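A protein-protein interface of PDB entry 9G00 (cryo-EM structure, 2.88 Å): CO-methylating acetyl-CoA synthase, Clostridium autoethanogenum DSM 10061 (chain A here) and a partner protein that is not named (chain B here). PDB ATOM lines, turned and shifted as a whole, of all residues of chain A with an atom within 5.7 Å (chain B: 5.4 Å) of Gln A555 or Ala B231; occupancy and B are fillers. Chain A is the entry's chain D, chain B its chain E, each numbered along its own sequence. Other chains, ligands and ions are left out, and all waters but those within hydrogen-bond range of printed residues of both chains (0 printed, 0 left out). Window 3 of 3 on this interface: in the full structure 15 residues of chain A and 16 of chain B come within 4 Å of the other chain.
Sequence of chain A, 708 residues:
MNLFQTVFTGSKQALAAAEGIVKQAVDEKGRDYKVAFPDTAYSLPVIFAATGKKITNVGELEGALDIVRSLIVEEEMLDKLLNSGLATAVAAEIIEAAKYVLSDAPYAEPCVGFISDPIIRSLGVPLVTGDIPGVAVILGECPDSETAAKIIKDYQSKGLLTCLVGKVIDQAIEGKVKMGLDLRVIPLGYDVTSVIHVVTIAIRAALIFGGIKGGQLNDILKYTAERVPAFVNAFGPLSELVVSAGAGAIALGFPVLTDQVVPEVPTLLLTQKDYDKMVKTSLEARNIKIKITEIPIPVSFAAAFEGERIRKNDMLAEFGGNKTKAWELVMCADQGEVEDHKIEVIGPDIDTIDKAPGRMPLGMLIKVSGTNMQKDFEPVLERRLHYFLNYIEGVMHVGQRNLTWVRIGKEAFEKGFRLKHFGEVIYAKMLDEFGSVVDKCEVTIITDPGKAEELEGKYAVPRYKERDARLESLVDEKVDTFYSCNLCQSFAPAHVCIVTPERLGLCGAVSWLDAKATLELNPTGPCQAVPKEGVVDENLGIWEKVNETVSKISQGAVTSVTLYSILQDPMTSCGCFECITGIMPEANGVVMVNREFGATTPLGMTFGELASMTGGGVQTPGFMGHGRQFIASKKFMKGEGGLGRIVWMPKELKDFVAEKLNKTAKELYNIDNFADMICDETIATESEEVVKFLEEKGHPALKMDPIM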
ATOM      1  N   GLN A 489      20.281 -28.532 -17.939  1.00  0.00           N
ATOM      2  CA  GLN A 489      19.974 -28.010 -19.262  1.00  0.00           C
ATOM      3  C   GLN A 489      20.763 -26.752 -19.598  1.00  0.00           C
ATOM      4  O   GLN A 489      20.663 -26.267 -20.728  1.00  0.00           O
ATOM      5  CB  GLN A 489      18.481 -27.725 -19.381  1.00  0.00           C
ATOM      6  CG  GLN A 489      17.635 -28.975 -19.397  1.00  0.00           C
ATOM      7  CD  GLN A 489      16.228 -28.713 -19.875  1.00  0.00           C
ATOM      8  OE1 GLN A 489      15.896 -27.604 -20.283  1.00  0.00           O
ATOM      9  NE2 GLN A 489      15.390 -29.735 -19.829  1.00  0.00           N
ATOM     10  N   VAL A 550       8.180 -35.351 -20.987  1.00  0.00           N
ATOM     11  CA  VAL A 550       9.561 -35.232 -21.442  1.00  0.00           C
ATOM     12  C   VAL A 550       9.640 -34.322 -22.660  1.00  0.00           C
ATOM     13  O   VAL A 550      10.557 -33.502 -22.775  1.00  0.00           O
ATOM     14  CB  VAL A 550      10.150 -36.628 -21.724  1.00  0.00           C
ATOM     15  CG1 VAL A 550      11.403 -36.537 -22.575  1.00  0.00           C
ATOM     16  CG2 VAL A 550      10.480 -37.322 -20.421  1.00  0.00           C
ATOM     17  N   SER A 551       8.690 -34.449 -23.587  1.00  0.00           N
ATOM     18  CA  SER A 551       8.667 -33.570 -24.750  1.00  0.00           C
ATOM     19  C   SER A 551       8.366 -32.127 -24.375  1.00  0.00           C
ATOM     20  O   SER A 551       8.691 -31.220 -25.147  1.00  0.00           O
ATOM     21  CB  SER A 551       7.639 -34.061 -25.767  1.00  0.00           C
ATOM     22  OG  SER A 551       6.334 -34.048 -25.222  1.00  0.00           O
ATOM     23  N   LYS A 552       7.749 -31.893 -23.220  1.00  0.00           N
ATOM     24  CA  LYS A 552       7.450 -30.530 -22.804  1.00  0.00           C
ATOM     25  C   LYS A 552       8.672 -29.871 -22.177  1.00  0.00           C
ATOM     26  O   LYS A 552       9.006 -28.729 -22.505  1.00  0.00           O
ATOM     27  CB  LYS A 552       6.279 -30.526 -21.819  1.00  0.00           C
ATOM     28  CG  LYS A 552       5.530 -29.206 -21.740  1.00  0.00           C
ATOM     29  CD  LYS A 552       4.685 -28.973 -22.987  1.00  0.00           C
ATOM     30  CE  LYS A 552       3.983 -27.618 -22.964  1.00  0.00           C
ATOM     31  NZ  LYS A 552       4.939 -26.475 -23.050  1.00  0.00           N
ATOM     32  N   ILE A 553       9.352 -30.582 -21.279  1.00  0.00           N
ATOM     33  CA  ILE A 553      10.499 -30.002 -20.590  1.00  0.00           C
ATOM     34  C   ILE A 553      11.675 -29.835 -21.540  1.00  0.00           C
ATOM     35  O   ILE A 553      12.374 -28.817 -21.508  1.00  0.00           O
ATOM     36  CB  ILE A 553      10.871 -30.860 -19.370  1.00  0.00           C
ATOM     37  CG1 ILE A 553       9.669 -30.973 -18.436  1.00  0.00           C
ATOM     38  CG2 ILE A 553      12.053 -30.245 -18.640  1.00  0.00           C
ATOM     39  CD1 ILE A 553       9.900 -31.857 -17.245  1.00  0.00           C
ATOM     40  N   SER A 554      11.921 -30.824 -22.391  1.00  0.00           N
ATOM     41  CA  SER A 554      13.016 -30.755 -23.349  1.00  0.00           C
ATOM     42  C   SER A 554      12.699 -29.857 -24.536  1.00  0.00           C
ATOM     43  O   SER A 554      13.509 -29.774 -25.463  1.00  0.00           O
ATOM     44  CB  SER A 554      13.374 -32.157 -23.842  1.00  0.00           C
ATOM     45  OG  SER A 554      12.262 -32.778 -24.454  1.00  0.00           O
ATOM     46  N   GLN A 555      11.557 -29.170 -24.518  1.00  0.00           N
ATOM     47  CA  GLN A 555      11.152 -28.294 -25.614  1.00  0.00           C
ATOM     48  C   GLN A 555      11.062 -29.063 -26.930  1.00  0.00           C
ATOM     49  O   GLN A 555      11.469 -28.576 -27.985  1.00  0.00           O
ATOM     50  CB  GLN A 555      12.105 -27.106 -25.749  1.00  0.00           C
ATOM     51  CG  GLN A 555      12.301 -26.314 -24.466  1.00  0.00           C
ATOM     52  CD  GLN A 555      11.026 -25.662 -23.974  1.00  0.00           C
ATOM     53  OE1 GLN A 555      10.044 -25.552 -24.706  1.00  0.00           O
ATOM     54  NE2 GLN A 555      11.033 -25.226 -22.721  1.00  0.00           N
ATOM     55  N   GLY A 556      10.535 -30.284 -26.860  1.00  0.00           N
ATOM     56  CA  GLY A 556      10.271 -31.079 -28.039  1.00  0.00           C
ATOM     57  C   GLY A 556      11.458 -31.815 -28.613  1.00  0.00           C
ATOM     58  O   GLY A 556      11.302 -32.503 -29.628  1.00  0.00           O
ATOM     59  N   ALA A 557      12.638 -31.698 -28.006  1.00  0.00           N
ATOM     60  CA  ALA A 557      13.807 -32.382 -28.544  1.00  0.00           C
ATOM     61  C   ALA A 557      13.682 -33.895 -28.397  1.00  0.00           C
ATOM     62  O   ALA A 557      14.000 -34.641 -29.329  1.00  0.00           O
ATOM     63  CB  ALA A 557      15.068 -31.878 -27.849  1.00  0.00           C
ATOM     64  N   ILE B 185      17.325 -20.218 -20.272  1.00  0.00           N
ATOM     65  CA  ILE B 185      15.914 -20.306 -20.653  1.00  0.00           C
ATOM     66  C   ILE B 185      15.057 -20.709 -19.458  1.00  0.00           C
ATOM     67  O   ILE B 185      13.921 -20.241 -19.310  1.00  0.00           O
ATOM     68  CB  ILE B 185      15.717 -21.284 -21.834  1.00  0.00           C
ATOM     69  CG1 ILE B 185      14.228 -21.403 -22.195  1.00  0.00           C
ATOM     70  CG2 ILE B 185      16.274 -22.658 -21.502  1.00  0.00           C
ATOM     71  CD1 ILE B 185      13.928 -22.321 -23.361  1.00  0.00           C
ATOM     72  N   LYS B 189      12.266 -18.634 -17.931  1.00  0.00           N
ATOM     73  CA  LYS B 189      10.947 -19.232 -17.782  1.00  0.00           C
ATOM     74  C   LYS B 189      10.450 -19.125 -16.344  1.00  0.00           C
ATOM     75  O   LYS B 189       9.254 -18.928 -16.111  1.00  0.00           O
ATOM     76  CB  LYS B 189      11.004 -20.687 -18.243  1.00  0.00           C
ATOM     77  CG  LYS B 189       9.671 -21.394 -18.316  1.00  0.00           C
ATOM     78  CD  LYS B 189       9.798 -22.689 -19.105  1.00  0.00           C
ATOM     79  CE  LYS B 189       8.577 -23.581 -18.946  1.00  0.00           C
ATOM     80  NZ  LYS B 189       8.409 -24.082 -17.551  1.00  0.00           N
ATOM     81  N   ASP B 226      18.252 -17.849 -28.972  1.00  0.00           N
ATOM     82  CA  ASP B 226      17.739 -18.847 -29.905  1.00  0.00           C
ATOM     83  C   ASP B 226      16.763 -19.790 -29.219  1.00  0.00           C
ATOM     84  O   ASP B 226      15.710 -20.116 -29.775  1.00  0.00           O
ATOM     85  CB  ASP B 226      18.889 -19.648 -30.514  1.00  0.00           C
ATOM     86  CG  ASP B 226      19.631 -18.886 -31.594  1.00  0.00           C
ATOM     87  OD1 ASP B 226      18.991 -18.100 -32.324  1.00  0.00           O
ATOM     88  OD2 ASP B 226      20.857 -19.084 -31.719  1.00  0.00           O
ATOM     89  N   ARG B 227      17.095 -20.235 -28.008  1.00  0.00           N
ATOM     90  CA  ARG B 227      16.263 -21.219 -27.324  1.00  0.00           C
ATOM     91  C   ARG B 227      14.909 -20.642 -26.933  1.00  0.00           C
ATOM     92  O   ARG B 227      13.879 -21.307 -27.093  1.00  0.00           O
ATOM     93  CB  ARG B 227      16.999 -21.756 -26.102  1.00  0.00           C
ATOM     94  CG  ARG B 227      18.136 -22.681 -26.464  1.00  0.00           C
ATOM     95  CD  ARG B 227      19.136 -22.826 -25.343  1.00  0.00           C
ATOM     96  NE  ARG B 227      18.613 -23.585 -24.217  1.00  0.00           N
ATOM     97  CZ  ARG B 227      19.335 -23.939 -23.164  1.00  0.00           C
ATOM     98  NH1 ARG B 227      20.620 -23.638 -23.075  1.00  0.00           N
ATOM     99  NH2 ARG B 227      18.754 -24.608 -22.173  1.00  0.00           N
ATOM    100  N   VAL B 228      14.880 -19.413 -26.419  1.00  0.00           N
ATOM    101  CA  VAL B 228      13.611 -18.832 -25.995  1.00  0.00           C
ATOM    102  C   VAL B 228      12.720 -18.557 -27.199  1.00  0.00           C
ATOM    103  O   VAL B 228      11.497 -18.708 -27.126  1.00  0.00           O
ATOM    104  CB  VAL B 228      13.842 -17.559 -25.160  1.00  0.00           C
ATOM    105  CG1 VAL B 228      14.601 -17.891 -23.890  1.00  0.00           C
ATOM    106  CG2 VAL B 228      14.577 -16.509 -25.963  1.00  0.00           C
ATOM    107  N   LYS B 229      13.310 -18.129 -28.315  1.00  0.00           N
ATOM    108  CA  LYS B 229      12.517 -17.879 -29.515  1.00  0.00           C
ATOM    109  C   LYS B 229      11.929 -19.168 -30.069  1.00  0.00           C
ATOM    110  O   LYS B 229      10.761 -19.203 -30.468  1.00  0.00           O
ATOM    111  CB  LYS B 229      13.365 -17.183 -30.576  1.00  0.00           C
ATOM    112  CG  LYS B 229      13.318 -15.667 -30.516  1.00  0.00           C
ATOM    113  CD  LYS B 229      11.987 -15.134 -31.006  1.00  0.00           C
ATOM    114  CE  LYS B 229      11.923 -13.624 -30.919  1.00  0.00           C
ATOM    115  NZ  LYS B 229      11.981 -13.140 -29.515  1.00  0.00           N
ATOM    116  N   LEU B 230      12.724 -20.239 -30.109  1.00  0.00           N
ATOM    117  CA  LEU B 230      12.220 -21.501 -30.638  1.00  0.00           C
ATOM    118  C   LEU B 230      11.174 -22.107 -29.713  1.00  0.00           C
ATOM    119  O   LEU B 230      10.190 -22.689 -30.180  1.00  0.00           O
ATOM    120  CB  LEU B 230      13.373 -22.476 -30.864  1.00  0.00           C
ATOM    121  CG  LEU B 230      14.321 -22.126 -32.013  1.00  0.00           C
ATOM    122  CD1 LEU B 230      15.487 -23.089 -32.045  1.00  0.00           C
ATOM    123  CD2 LEU B 230      13.591 -22.140 -33.346  1.00  0.00           C
ATOM    124  N   ALA B 231      11.377 -22.001 -28.400  1.00  0.00           N
ATOM    125  CA  ALA B 231      10.389 -22.524 -27.462  1.00  0.00           C
ATOM    126  C   ALA B 231       9.093 -21.727 -27.525  1.00  0.00           C
ATOM    127  O   ALA B 231       8.002 -22.301 -27.463  1.00  0.00           O
ATOM    128  CB  ALA B 231      10.951 -22.510 -26.045  1.00  0.00           C
ATOM    129  N   ALA B 232       9.191 -20.403 -27.647  1.00  0.00           N
ATOM    130  CA  ALA B 232       7.992 -19.572 -27.667  1.00  0.00           C
ATOM    131  C   ALA B 232       7.150 -19.838 -28.905  1.00  0.00           C
ATOM    132  O   ALA B 232       5.917 -19.880 -28.827  1.00  0.00           O
ATOM    133  CB  ALA B 232       8.376 -18.097 -27.597  1.00  0.00           C
ATOM    134  N   LEU B 233       7.791 -20.011 -30.056  1.00  0.00           N
ATOM    135  CA  LEU B 233       7.090 -20.191 -31.319  1.00  0.00           C
ATOM    136  C   LEU B 233       6.922 -21.658 -31.692  1.00  0.00           C
ATOM    137  O   LEU B 233       5.805 -22.102 -31.968  1.00  0.00           O
ATOM    138  CB  LEU B 233       7.839 -19.457 -32.437  1.00  0.00           C
ATOM    139  CG  LEU B 233       8.130 -17.979 -32.187  1.00  0.00           C
ATOM    140  CD1 LEU B 233       9.042 -17.442 -33.257  1.00  0.00           C
ATOM    141  CD2 LEU B 233       6.847 -17.182 -32.147  1.00  0.00           C
ATOM    142  N   GLY B 234       8.012 -22.423 -31.703  1.00  0.00           N
ATOM    143  CA  GLY B 234       7.916 -23.817 -32.104  1.00  0.00           C
ATOM    144  C   GLY B 234       7.102 -24.658 -31.140  1.00  0.00           C
ATOM    145  O   GLY B 234       6.276 -25.472 -31.560  1.00  0.00           O
ATOM    146  N   GLN B 235       7.307 -24.463 -29.841  1.00  0.00           N
ATOM    147  CA  GLN B 235       6.628 -25.230 -28.809  1.00  0.00           C
ATOM    148  C   GLN B 235       5.414 -24.514 -28.242  1.00  0.00           C
ATOM    149  O   GLN B 235       4.766 -25.046 -27.335  1.00  0.00           O
ATOM    150  CB  GLN B 235       7.603 -25.557 -27.677  1.00  0.00           C
ATOM    151  CG  GLN B 235       8.934 -26.087 -28.159  1.00  0.00           C
ATOM    152  CD  GLN B 235       8.787 -27.319 -29.018  1.00  0.00           C
ATOM    153  OE1 GLN B 235       8.081 -28.257 -28.657  1.00  0.00           O
ATOM    154  NE2 GLN B 235       9.451 -27.323 -30.167  1.00  0.00           N
ATOM    155  N   ASP B 236       5.097 -23.324 -28.742  1.00  0.00           N
ATOM    156  CA  ASP B 236       3.935 -22.571 -28.286  1.00  0.00           C
ATOM    157  C   ASP B 236       3.941 -22.421 -26.769  1.00  0.00           C
ATOM    158  O   ASP B 236       2.919 -22.579 -26.100  1.00  0.00           O
ATOM    159  CB  ASP B 236       2.643 -23.235 -28.757  1.00  0.00           C
ATOM    160  CG  ASP B 236       1.472 -22.281 -28.769  1.00  0.00           C
ATOM    161  OD1 ASP B 236       1.690 -21.065 -28.588  1.00  0.00           O
ATOM    162  OD2 ASP B 236       0.331 -22.746 -28.959  1.00  0.00           O
ATOM    163  N   ASP B 237       5.115 -22.123 -26.221  1.00  0.00           N
ATOM    164  CA  ASP B 237       5.272 -21.957 -24.782  1.00  0.00           C
ATOM    165  C   ASP B 237       4.700 -20.603 -24.381  1.00  0.00           C
ATOM    166  O   ASP B 237       5.260 -19.559 -24.728  1.00  0.00           O
ATOM    167  CB  ASP B 237       6.745 -22.066 -24.403  1.00  0.00           C
ATOM    168  CG  ASP B 237       6.945 -22.396 -22.948  1.00  0.00           C
ATOM    169  OD1 ASP B 237       5.947 -22.698 -22.264  1.00  0.00           O
ATOM    170  OD2 ASP B 237       8.102 -22.355 -22.486  1.00  0.00           O
ATOM    171  N   LEU B 240       6.917 -17.953 -22.404  1.00  0.00           N
ATOM    172  CA  LEU B 240       8.053 -17.317 -23.051  1.00  0.00           C
ATOM    173  C   LEU B 240       7.646 -16.396 -24.189  1.00  0.00           C
ATOM    174  O   LEU B 240       8.523 -15.794 -24.819  1.00  0.00           O
ATOM    175  CB  LEU B 240       9.026 -18.375 -23.587  1.00  0.00           C
ATOM    176  CG  LEU B 240       9.796 -19.191 -22.553  1.00  0.00           C
ATOM    177  CD1 LEU B 240      10.664 -20.211 -23.243  1.00  0.00           C
ATOM    178  CD2 LEU B 240      10.644 -18.301 -21.675  1.00  0.00           C
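The backbone carbonyl oxygen (O) of Ser A551 is in hydrogen-bond range of the backbone NH (N) of Gly A556 (2.7 Å). The backbone carbonyl oxygen of Leu B230 sits at hydrogen-bond distance from the backbone NH of Gln B235 (3.4 Å). O of Ala B231 is in hydrogen-bond range of N of Asp B236, 3.3 Å away. The backbone carbonyl oxygen (O) of Ala B231 is in hydrogen-bond range of the backbone NH (N) of Asp B237.
O of Gln A489 lies within hydrogen-bond range of NH2 of Arg B227 (2.9 Å). The side-chain amino group (NZ) of Lys A552 lies within salt-bridge range of the side-chain carboxylate (OD1) of Asp B237 (3.99 Å). The backbone carbonyl oxygen (O) of Gln A555 lies close to the side-chain amide nitrogen (NE2) of Gln B235, at 3.2 Å.
Printed residues of chain B that touch a printed residue of chain A: Arg B227, Ala B231, Gln B235 and Asp B237. Hydrophobic or aromatic side chains of chain B within 4 Å of the printed part of chain A: Ala B231. Among the printed residues, Asp or Glu carboxylates within 4 Å of a Lys or Arg side-chain nitrogen of the other chain: Lys A552 with Asp B237 (3.99 Å).
Printed residues of chain B within 4 Å of Gln A489: Arg B227 (2.9 Å). Val A550 touches none of the printed residues of chain B. Printed residues of chain B within 4 Å of Lys A552: Asp B237. Of chain B, only Ala B231 and Gln B235 come within 4 Å of Gln A555. Printed residues of chain B within 4 Å of Gly A556: Gln B235. Ala B231 touches just one residue of chain A: Gln A555. Leu B233 touches none of the printed residues of chain A. Printed residues of chain A within 4 Å of Asp B237: Lys A552. The nearest printed residue of chain A that does not touch Ala B231 is Lys A552 (6.8 Å). The nearest printed residue of chain A that does not touch Arg B227 is Gln A555 (5.9 Å).
Among the printed residues, merely in contact across the chains: Gln A555 with Ala B231 and Gly A556 with Gln B235.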
